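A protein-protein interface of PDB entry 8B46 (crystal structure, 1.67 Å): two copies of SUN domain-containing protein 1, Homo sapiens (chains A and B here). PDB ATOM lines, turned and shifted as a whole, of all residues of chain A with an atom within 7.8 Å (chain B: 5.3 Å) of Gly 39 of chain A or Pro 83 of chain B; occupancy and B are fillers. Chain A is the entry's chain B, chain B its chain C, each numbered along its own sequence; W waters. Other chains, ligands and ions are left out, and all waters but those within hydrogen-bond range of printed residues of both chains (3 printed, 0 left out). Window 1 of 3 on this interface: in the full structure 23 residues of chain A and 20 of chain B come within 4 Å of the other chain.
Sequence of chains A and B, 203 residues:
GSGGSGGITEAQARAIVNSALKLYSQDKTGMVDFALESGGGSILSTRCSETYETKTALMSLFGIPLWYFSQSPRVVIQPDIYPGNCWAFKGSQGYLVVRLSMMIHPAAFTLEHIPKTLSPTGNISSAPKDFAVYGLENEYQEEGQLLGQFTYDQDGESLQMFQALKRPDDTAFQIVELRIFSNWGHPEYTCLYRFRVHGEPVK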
ATOM      1  N   ASP A  27      14.844  -9.947  -2.617  1.00  0.00           N
ATOM      2  CA  ASP A  27      14.911  -9.416  -3.979  1.00  0.00           C
ATOM      3  C   ASP A  27      14.002  -8.201  -4.141  1.00  0.00           C
ATOM      4  O   ASP A  27      13.426  -7.982  -5.203  1.00  0.00           O
ATOM      5  CB  ASP A  27      14.553 -10.520  -5.000  1.00  0.00           C
ATOM      6  CG  ASP A  27      15.039 -10.229  -6.416  1.00  0.00           C
ATOM      7  OD1 ASP A  27      15.847  -9.274  -6.639  1.00  0.00           O
ATOM      8  OD2 ASP A  27      14.617 -11.000  -7.342  1.00  0.00           O
ATOM      9  N   MET A  31       8.768 -11.897  -4.334  1.00  0.00           N
ATOM     10  CA  MET A  31       8.074 -12.673  -5.366  1.00  0.00           C
ATOM     11  C   MET A  31       9.085 -13.399  -6.237  1.00  0.00           C
ATOM     12  O   MET A  31      10.097 -12.816  -6.623  1.00  0.00           O
ATOM     13  CB  MET A  31       7.253 -11.774  -6.272  1.00  0.00           C
ATOM     14  CG  MET A  31       6.073 -11.121  -5.575  1.00  0.00           C
ATOM     15  SD  MET A  31       5.294  -9.956  -6.708  1.00  0.00           S
ATOM     16  CE  MET A  31       3.852  -9.513  -5.739  1.00  0.00           C
ATOM     17  N   VAL A  32       8.767 -14.643  -6.620  1.00  0.00           N
ATOM     18  CA  VAL A  32       9.625 -15.370  -7.556  1.00  0.00           C
ATOM     19  C   VAL A  32       9.799 -14.556  -8.837  1.00  0.00           C
ATOM     20  O   VAL A  32       8.824 -14.032  -9.390  1.00  0.00           O
ATOM     21  CB  VAL A  32       8.997 -16.726  -7.912  1.00  0.00           C
ATOM     22  CG1 VAL A  32       9.892 -17.476  -8.895  1.00  0.00           C
ATOM     23  CG2 VAL A  32       8.683 -17.558  -6.686  1.00  0.00           C
ATOM     24  N   ASP A  33      11.036 -14.465  -9.321  1.00  0.00           N
ATOM     25  CA  ASP A  33      11.343 -13.937 -10.649  1.00  0.00           C
ATOM     26  C   ASP A  33      11.644 -15.154 -11.528  1.00  0.00           C
ATOM     27  O   ASP A  33      12.732 -15.748 -11.460  1.00  0.00           O
ATOM     28  CB  ASP A  33      12.507 -12.945 -10.622  1.00  0.00           C
ATOM     29  CG  ASP A  33      12.941 -12.511 -12.045  1.00  0.00           C
ATOM     30  OD1 ASP A  33      12.161 -12.795 -13.006  1.00  0.00           O
ATOM     31  OD2 ASP A  33      14.039 -11.901 -12.194  1.00  0.00           O
ATOM     32  N   PHE A  34      10.675 -15.521 -12.371  1.00  0.00           N
ATOM     33  CA  PHE A  34      10.885 -16.675 -13.235  1.00  0.00           C
ATOM     34  C   PHE A  34      11.829 -16.379 -14.394  1.00  0.00           C
ATOM     35  O   PHE A  34      12.245 -17.322 -15.075  1.00  0.00           O
ATOM     36  CB  PHE A  34       9.558 -17.157 -13.785  1.00  0.00           C
ATOM     37  CG  PHE A  34       8.697 -17.768 -12.749  1.00  0.00           C
ATOM     38  CD1 PHE A  34       8.879 -19.106 -12.389  1.00  0.00           C
ATOM     39  CD2 PHE A  34       7.762 -17.000 -12.069  1.00  0.00           C
ATOM     40  CE1 PHE A  34       8.083 -19.696 -11.417  1.00  0.00           C
ATOM     41  CE2 PHE A  34       6.988 -17.570 -11.070  1.00  0.00           C
ATOM     42  CZ  PHE A  34       7.135 -18.914 -10.741  1.00  0.00           C
ATOM     43  N   ALA A  35      12.169 -15.107 -14.631  1.00  0.00           N
ATOM     44  CA  ALA A  35      13.134 -14.748 -15.665  1.00  0.00           C
ATOM     45  C   ALA A  35      14.571 -14.787 -15.157  1.00  0.00           C
ATOM     46  O   ALA A  35      15.508 -14.801 -15.965  1.00  0.00           O
ATOM     47  CB  ALA A  35      12.819 -13.340 -16.208  1.00  0.00           C
ATOM     48  N   LEU A  36      14.769 -14.811 -13.841  1.00  0.00           N
ATOM     49  CA  LEU A  36      16.095 -14.652 -13.267  1.00  0.00           C
ATOM     50  C   LEU A  36      17.025 -15.732 -13.801  1.00  0.00           C
ATOM     51  O   LEU A  36      16.711 -16.918 -13.695  1.00  0.00           O
ATOM     52  CB  LEU A  36      16.004 -14.739 -11.734  1.00  0.00           C
ATOM     53  CG  LEU A  36      17.355 -14.538 -10.978  1.00  0.00           C
ATOM     54  CD1 LEU A  36      17.803 -13.060 -11.001  1.00  0.00           C
ATOM     55  CD2 LEU A  36      17.216 -15.075  -9.522  1.00  0.00           C
ATOM     56  N   GLU A  37      18.200 -15.336 -14.322  1.00  0.00           N
ATOM     57  CA  GLU A  37      19.061 -16.325 -14.986  1.00  0.00           C
ATOM     58  C   GLU A  37      19.545 -17.416 -14.017  1.00  0.00           C
ATOM     59  O   GLU A  37      19.470 -18.614 -14.322  1.00  0.00           O
ATOM     60  CB  GLU A  37      20.259 -15.623 -15.638  1.00  0.00           C
ATOM     61  CG  GLU A  37      21.031 -16.596 -16.520  1.00  0.00           C
ATOM     62  CD  GLU A  37      22.185 -15.872 -17.236  1.00  0.00           C
ATOM     63  OE1 GLU A  37      23.107 -15.390 -16.541  1.00  0.00           O
ATOM     64  OE2 GLU A  37      22.128 -15.743 -18.489  1.00  0.00           O
ATOM     65  N   SER A  38      20.035 -17.026 -12.830  1.00  0.00           N
ATOM     66  CA  SER A  38      20.591 -18.031 -11.927  1.00  0.00           C
ATOM     67  C   SER A  38      19.513 -19.005 -11.480  1.00  0.00           C
ATOM     68  O   SER A  38      19.806 -20.173 -11.240  1.00  0.00           O
ATOM     69  CB  SER A  38      21.264 -17.374 -10.704  1.00  0.00           C
ATOM     70  OG  SER A  38      20.300 -16.630  -9.945  1.00  0.00           O
ATOM     71  N   GLY A  39      18.245 -18.575 -11.438  1.00  0.00           N
ATOM     72  CA  GLY A  39      17.145 -19.470 -11.102  1.00  0.00           C
ATOM     73  C   GLY A  39      16.624 -20.318 -12.252  1.00  0.00           C
ATOM     74  O   GLY A  39      15.677 -21.088 -12.057  1.00  0.00           O
ATOM     75  N   GLY A  40      17.196 -20.197 -13.460  1.00  0.00           N
ATOM     76  CA  GLY A  40      16.761 -21.029 -14.566  1.00  0.00           C
ATOM     77  C   GLY A  40      16.211 -20.284 -15.739  1.00  0.00           C
ATOM     78  O   GLY A  40      15.870 -20.929 -16.740  1.00  0.00           O
ATOM     79  N   GLY A  41      16.090 -18.964 -15.681  1.00  0.00           N
ATOM     80  CA  GLY A  41      15.691 -18.219 -16.858  1.00  0.00           C
ATOM     81  C   GLY A  41      16.849 -18.087 -17.819  1.00  0.00           C
ATOM     82  O   GLY A  41      17.990 -18.320 -17.431  1.00  0.00           O
ATOM     83  N   SER A  42      16.554 -17.779 -19.093  1.00  0.00           N
ATOM     84  CA  SER A  42      17.636 -17.599 -20.048  1.00  0.00           C
ATOM     85  C   SER A  42      17.223 -16.630 -21.158  1.00  0.00           C
ATOM     86  O   SER A  42      16.052 -16.552 -21.550  1.00  0.00           O
ATOM     87  CB  SER A  42      18.076 -18.945 -20.636  1.00  0.00           C
ATOM     88  OG  SER A  42      16.976 -19.567 -21.242  1.00  0.00           O
ATOM     89  N   ILE A  77      18.789 -10.170 -16.991  1.00  0.00           N
ATOM     90  CA  ILE A  77      18.163 -11.096 -16.048  1.00  0.00           C
ATOM     91  C   ILE A  77      19.182 -11.439 -14.964  1.00  0.00           C
ATOM     92  O   ILE A  77      19.183 -12.554 -14.402  1.00  0.00           O
ATOM     93  CB  ILE A  77      17.563 -12.330 -16.768  1.00  0.00           C
ATOM     94  CG1 ILE A  77      18.550 -13.005 -17.754  1.00  0.00           C
ATOM     95  CG2 ILE A  77      16.353 -11.915 -17.562  1.00  0.00           C
ATOM     96  CD1 ILE A  77      18.018 -14.357 -18.280  1.00  0.00           C
ATOM     97  N   LEU A 100      11.492 -18.700 -19.477  1.00  0.00           N
ATOM     98  CA  LEU A 100      11.316 -18.672 -18.034  1.00  0.00           C
ATOM     99  C   LEU A 100      11.773 -19.998 -17.417  1.00  0.00           C
ATOM    100  O   LEU A 100      11.951 -21.005 -18.103  1.00  0.00           O
ATOM    101  CB  LEU A 100       9.850 -18.406 -17.679  1.00  0.00           C
ATOM    102  CG  LEU A 100       9.220 -17.153 -18.322  1.00  0.00           C
ATOM    103  CD1 LEU A 100       7.686 -17.080 -17.932  1.00  0.00           C
ATOM    104  CD2 LEU A 100       9.997 -15.886 -17.914  1.00  0.00           C
ATOM    105  N   SER A 101      11.966 -19.990 -16.101  1.00  0.00           N
ATOM    106  CA  SER A 101      12.422 -21.198 -15.421  1.00  0.00           C
ATOM    107  C   SER A 101      11.323 -22.237 -15.305  1.00  0.00           C
ATOM    108  O   SER A 101      11.619 -23.407 -15.056  1.00  0.00           O
ATOM    109  CB  SER A 101      12.981 -20.847 -14.036  1.00  0.00           C
ATOM    110  OG  SER A 101      11.978 -20.230 -13.252  1.00  0.00           O
ATOM    111  N   MET A 102      10.061 -21.849 -15.475  1.00  0.00           N
ATOM    112  CA  MET A 102       8.942 -22.771 -15.422  1.00  0.00           C
ATOM    113  C   MET A 102       7.854 -22.257 -16.345  1.00  0.00           C
ATOM    114  O   MET A 102       7.847 -21.080 -16.721  1.00  0.00           O
ATOM    115  CB  MET A 102       8.396 -22.923 -13.998  1.00  0.00           C
ATOM    116  CG  MET A 102       9.361 -23.590 -13.043  1.00  0.00           C
ATOM    117  SD  MET A 102       8.523 -23.900 -11.515  1.00  0.00           S
ATOM    118  CE  MET A 102       7.295 -25.094 -12.027  1.00  0.00           C
ATOM    119  N   ARG A 194      17.069  -4.329 -15.600  1.00  0.00           N
ATOM    120  CA  ARG A 194      16.574  -5.629 -15.140  1.00  0.00           C
ATOM    121  C   ARG A 194      15.095  -5.755 -15.433  1.00  0.00           C
ATOM    122  O   ARG A 194      14.308  -4.822 -15.186  1.00  0.00           O
ATOM    123  CB  ARG A 194      16.806  -5.874 -13.642  1.00  0.00           C
ATOM    124  CG  ARG A 194      16.373  -7.317 -13.265  1.00  0.00           C
ATOM    125  CD  ARG A 194      16.840  -7.750 -11.932  1.00  0.00           C
ATOM    126  NE  ARG A 194      16.270  -9.051 -11.584  1.00  0.00           N
ATOM    127  CZ  ARG A 194      16.109  -9.441 -10.327  1.00  0.00           C
ATOM    128  NH1 ARG A 194      16.533  -8.697  -9.318  1.00  0.00           N
ATOM    129  NH2 ARG A 194      15.485 -10.594 -10.070  1.00  0.00           N
ATOM    130  N   ILE B  81      23.311 -15.210  -2.664  1.00  0.00           N
ATOM    131  CA  ILE B  81      22.326 -16.271  -2.430  1.00  0.00           C
ATOM    132  C   ILE B  81      21.051 -16.058  -3.242  1.00  0.00           C
ATOM    133  O   ILE B  81      19.954 -16.384  -2.792  1.00  0.00           O
ATOM    134  CB  ILE B  81      21.936 -16.454  -0.942  1.00  0.00           C
ATOM    135  CG1 ILE B  81      21.343 -15.188  -0.363  1.00  0.00           C
ATOM    136  CG2 ILE B  81      23.140 -16.805  -0.047  1.00  0.00           C
ATOM    137  CD1 ILE B  81      20.495 -15.571   0.906  1.00  0.00           C
ATOM    138  N   TYR B  82      21.156 -15.463  -4.408  1.00  0.00           N
ATOM    139  CA  TYR B  82      20.011 -15.536  -5.313  1.00  0.00           C
ATOM    140  C   TYR B  82      19.720 -16.993  -5.672  1.00  0.00           C
ATOM    141  O   TYR B  82      20.644 -17.823  -5.684  1.00  0.00           O
ATOM    142  CB  TYR B  82      20.316 -14.747  -6.578  1.00  0.00           C
ATOM    143  CG  TYR B  82      20.006 -13.290  -6.389  1.00  0.00           C
ATOM    144  CD1 TYR B  82      20.893 -12.438  -5.731  1.00  0.00           C
ATOM    145  CD2 TYR B  82      18.774 -12.783  -6.794  1.00  0.00           C
ATOM    146  CE1 TYR B  82      20.576 -11.050  -5.538  1.00  0.00           C
ATOM    147  CE2 TYR B  82      18.444 -11.420  -6.603  1.00  0.00           C
ATOM    148  CZ  TYR B  82      19.333 -10.579  -5.948  1.00  0.00           C
ATOM    149  OH  TYR B  82      18.973  -9.252  -5.795  1.00  0.00           O
ATOM    150  N   PRO B  83      18.468 -17.324  -6.010  1.00  0.00           N
ATOM    151  CA  PRO B  83      18.130 -18.704  -6.393  1.00  0.00           C
ATOM    152  C   PRO B  83      19.103 -19.255  -7.422  1.00  0.00           C
ATOM    153  O   PRO B  83      19.388 -18.622  -8.452  1.00  0.00           O
ATOM    154  CB  PRO B  83      16.711 -18.570  -6.986  1.00  0.00           C
ATOM    155  CG  PRO B  83      16.111 -17.419  -6.210  1.00  0.00           C
ATOM    156  CD  PRO B  83      17.270 -16.451  -5.966  1.00  0.00           C
ATOM    157  N   GLY B  84      19.597 -20.463  -7.150  1.00  0.00           N
ATOM    158  CA  GLY B  84      20.575 -21.122  -8.004  1.00  0.00           C
ATOM    159  C   GLY B  84      22.026 -20.911  -7.605  1.00  0.00           C
ATOM    160  O   GLY B  84      22.894 -21.662  -8.058  1.00  0.00           O
ATOM    161  N   ASN B  85      22.326 -19.930  -6.753  1.00  0.00           N
ATOM    162  CA  ASN B  85      23.714 -19.685  -6.345  1.00  0.00           C
ATOM    163  C   ASN B  85      24.058 -20.569  -5.146  1.00  0.00           C
ATOM    164  O   ASN B  85      24.348 -20.095  -4.040  1.00  0.00           O
ATOM    165  CB  ASN B  85      23.904 -18.220  -5.985  1.00  0.00           C
ATOM    166  CG  ASN B  85      23.784 -17.297  -7.164  1.00  0.00           C
ATOM    167  OD1 ASN B  85      24.072 -17.650  -8.287  1.00  0.00           O
ATOM    168  ND2 ASN B  85      23.307 -16.109  -6.900  1.00  0.00           N
ATOM    169  N   ILE B 114      17.343 -19.979   0.256  1.00  0.00           N
ATOM    170  CA  ILE B 114      16.372 -18.998  -0.239  1.00  0.00           C
ATOM    171  C   ILE B 114      15.052 -19.184   0.506  1.00  0.00           C
ATOM    172  O   ILE B 114      14.713 -20.313   0.893  1.00  0.00           O
ATOM    173  CB  ILE B 114      16.167 -19.100  -1.753  1.00  0.00           C
ATOM    174  CG1 ILE B 114      15.717 -20.526  -2.146  1.00  0.00           C
ATOM    175  CG2 ILE B 114      17.450 -18.555  -2.476  1.00  0.00           C
ATOM    176  CD1 ILE B 114      15.148 -20.564  -3.552  1.00  0.00           C
ATOM    177  N   LEU B 118      10.700 -17.047  -2.849  1.00  0.00           N
ATOM    178  CA  LEU B 118      11.540 -16.820  -4.021  1.00  0.00           C
ATOM    179  C   LEU B 118      11.829 -18.101  -4.809  1.00  0.00           C
ATOM    180  O   LEU B 118      12.528 -18.052  -5.828  1.00  0.00           O
ATOM    181  CB  LEU B 118      12.856 -16.164  -3.601  1.00  0.00           C
ATOM    182  CG  LEU B 118      12.691 -14.761  -3.005  1.00  0.00           C
ATOM    183  CD1 LEU B 118      14.071 -14.204  -2.749  1.00  0.00           C
ATOM    184  CD2 LEU B 118      11.915 -13.868  -3.924  1.00  0.00           C
ATOM    185  N   PRO B 120      10.987 -21.038  -7.349  1.00  0.00           N
ATOM    186  CA  PRO B 120      10.008 -21.192  -8.436  1.00  0.00           C
ATOM    187  C   PRO B 120       8.917 -22.225  -8.158  1.00  0.00           C
ATOM    188  O   PRO B 120       7.746 -22.006  -8.509  1.00  0.00           O
ATOM    189  CB  PRO B 120      10.892 -21.620  -9.605  1.00  0.00           C
ATOM    190  CG  PRO B 120      12.254 -21.042  -9.280  1.00  0.00           C
ATOM    191  CD  PRO B 120      12.381 -21.161  -7.798  1.00  0.00           C
ATOM    192  N   TYR B 193      23.223 -23.052   0.122  1.00  0.00           N
ATOM    193  CA  TYR B 193      23.454 -21.716  -0.375  1.00  0.00           C
ATOM    194  C   TYR B 193      24.641 -21.034   0.315  1.00  0.00           C
ATOM    195  O   TYR B 193      25.499 -20.477  -0.350  1.00  0.00           O
ATOM    196  CB  TYR B 193      22.183 -20.872  -0.207  1.00  0.00           C
ATOM    197  CG  TYR B 193      21.230 -21.065  -1.359  1.00  0.00           C
ATOM    198  CD1 TYR B 193      20.296 -22.136  -1.364  1.00  0.00           C
ATOM    199  CD2 TYR B 193      21.310 -20.203  -2.466  1.00  0.00           C
ATOM    200  CE1 TYR B 193      19.450 -22.359  -2.474  1.00  0.00           C
ATOM    201  CE2 TYR B 193      20.459 -20.372  -3.565  1.00  0.00           C
ATOM    202  CZ  TYR B 193      19.510 -21.464  -3.534  1.00  0.00           C
ATOM    203  OH  TYR B 193      18.675 -21.670  -4.622  1.00  0.00           O
HETATM  204  O   HOH W   1      17.056  -6.766  -6.313  1.00  0.00           O
HETATM  205  O   HOH W   2      17.991  -9.596  -3.066  1.00  0.00           O
HETATM  206  O   HOH W   3      13.142 -15.849  -7.698  1.00  0.00           O
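Of the printed residues of chain B, Val 32 of chain A touches Leu 118 and Pro 120. Of the printed residues of chain B, Leu 36 of chain A touches Tyr 82 and Pro 83. Gly 39 of chain A touches just one residue of chain B: Pro 83. Pro 83 of chain B touches just these residues of chain A: Leu 36 (3.8 Å), Ser 38 (2.7 Å) and Gly 39 (3.2 Å). Printed residues of chain A within 4 Å of Gly 84 of chain B: Ser 38. Of the printed residues of chain A, Leu 118 of chain B touches Met 31 (3.4 Å) and Val 32 (3.7 Å). Printed residues of chain A within 4 Å of Pro 120 of chain B: Val 32 (3.7 Å), Phe 34 (3.7 Å) and Met 102 (3.6 Å). The nearest printed residue of chain B that does not touch Phe 34 of chain A is Leu 118 of chain B (7.3 Å).
Among the printed residues, pairs that only touch across the chains: Met 31 of chain A with Leu 118 of chain B, Val 32 of chain A with Leu 118 of chain B, Val 32 of chain A with Pro 120 of chain B, Phe 34 of chain A with Pro 120 of chain B, Leu 36 of chain A with Tyr 82 of chain B, Leu 36 of chain A with Pro 83 of chain B, Ser 38 of chain A with Tyr 82 of chain B, Ser 38 of chain A with Gly 84 of chain B and Ser 38 of chain A with Asn 85 of chain B.
O of Pro 83 of chain B sits at hydrogen-bond distance from N of Gly 39 of chain A (3.2 Å). The side-chain carboxylate (OD1) of Asp 27 of chain A is in hydrogen-bond range of the side-chain hydroxyl (OH) of Tyr 82 of chain B. The backbone carbonyl oxygen of Pro 120 of chain B lies close to the side-chain sulfur of Met 102 of chain A. OG of Ser 38 of chain A is in hydrogen-bond range of O of Pro 83 of chain B (2.7 Å).
Water W1 bridges the side-chain carboxylate (OD1) of Asp 27 of chain A (2.8 Å) and the side-chain hydroxyl (OH) of Tyr 82 of chain B (3.2 Å). Water W2 lies within hydrogen-bond range of the side-chain hydroxyl (OH) of Tyr 82 of chain B (2.9 Å) and the backbone NH (N) of Asp 27 of chain A (3.2 Å). Water W3 bridges O of Leu 118 of chain B (3.0 Å) and N of Asp 33 of chain A (3.0 Å).
No position is printed for both chains. Of the 13 pairs that touch across the chains among the printed residues, none has its exchanged pair printed and touching as well.
The backbone NH of Gly 84 of chain B is in hydrogen-bond range of the side-chain hydroxyl of Tyr 193 of chain B (2.9 Å). The backbone carbonyl oxygen (O) of Leu 36 of chain A sits at hydrogen-bond distance from the backbone NH (N) of Gly 41 of chain A (2.9 Å). The backbone NH of Tyr 82 of chain B lies close to the side-chain amide nitrogen of Asn 85 of chain B. The side-chain carboxylate of Asp 27 of chain A lies within salt-bridge range of the guanidinium group of Arg 194 of chain A, at 2.8 Å. The backbone NH (N) of Ser 101 of chain A is in hydrogen-bond range of the backbone carbonyl oxygen (O) of Phe 34 of chain A (2.9 Å). The side-chain carboxylate (OD1) of Asp 33 of chain A lies within hydrogen-bond range of the backbone NH (N) of Leu 36 of chain A.
Printed residues of chain A that touch a printed residue of chain B: Asp 27, Met 31, Val 32, Phe 34, Leu 36, Ser 38, Gly 39 and Met 102. Of the 9 printed residues of chain B, 6 touch a printed residue of chain A. Among the printed residues, 13 pairs touch across the chains. Among the printed residues, no Asp or Glu carboxylate lies within 4 Å of a Lys or Arg side-chain nitrogen of the other chain.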
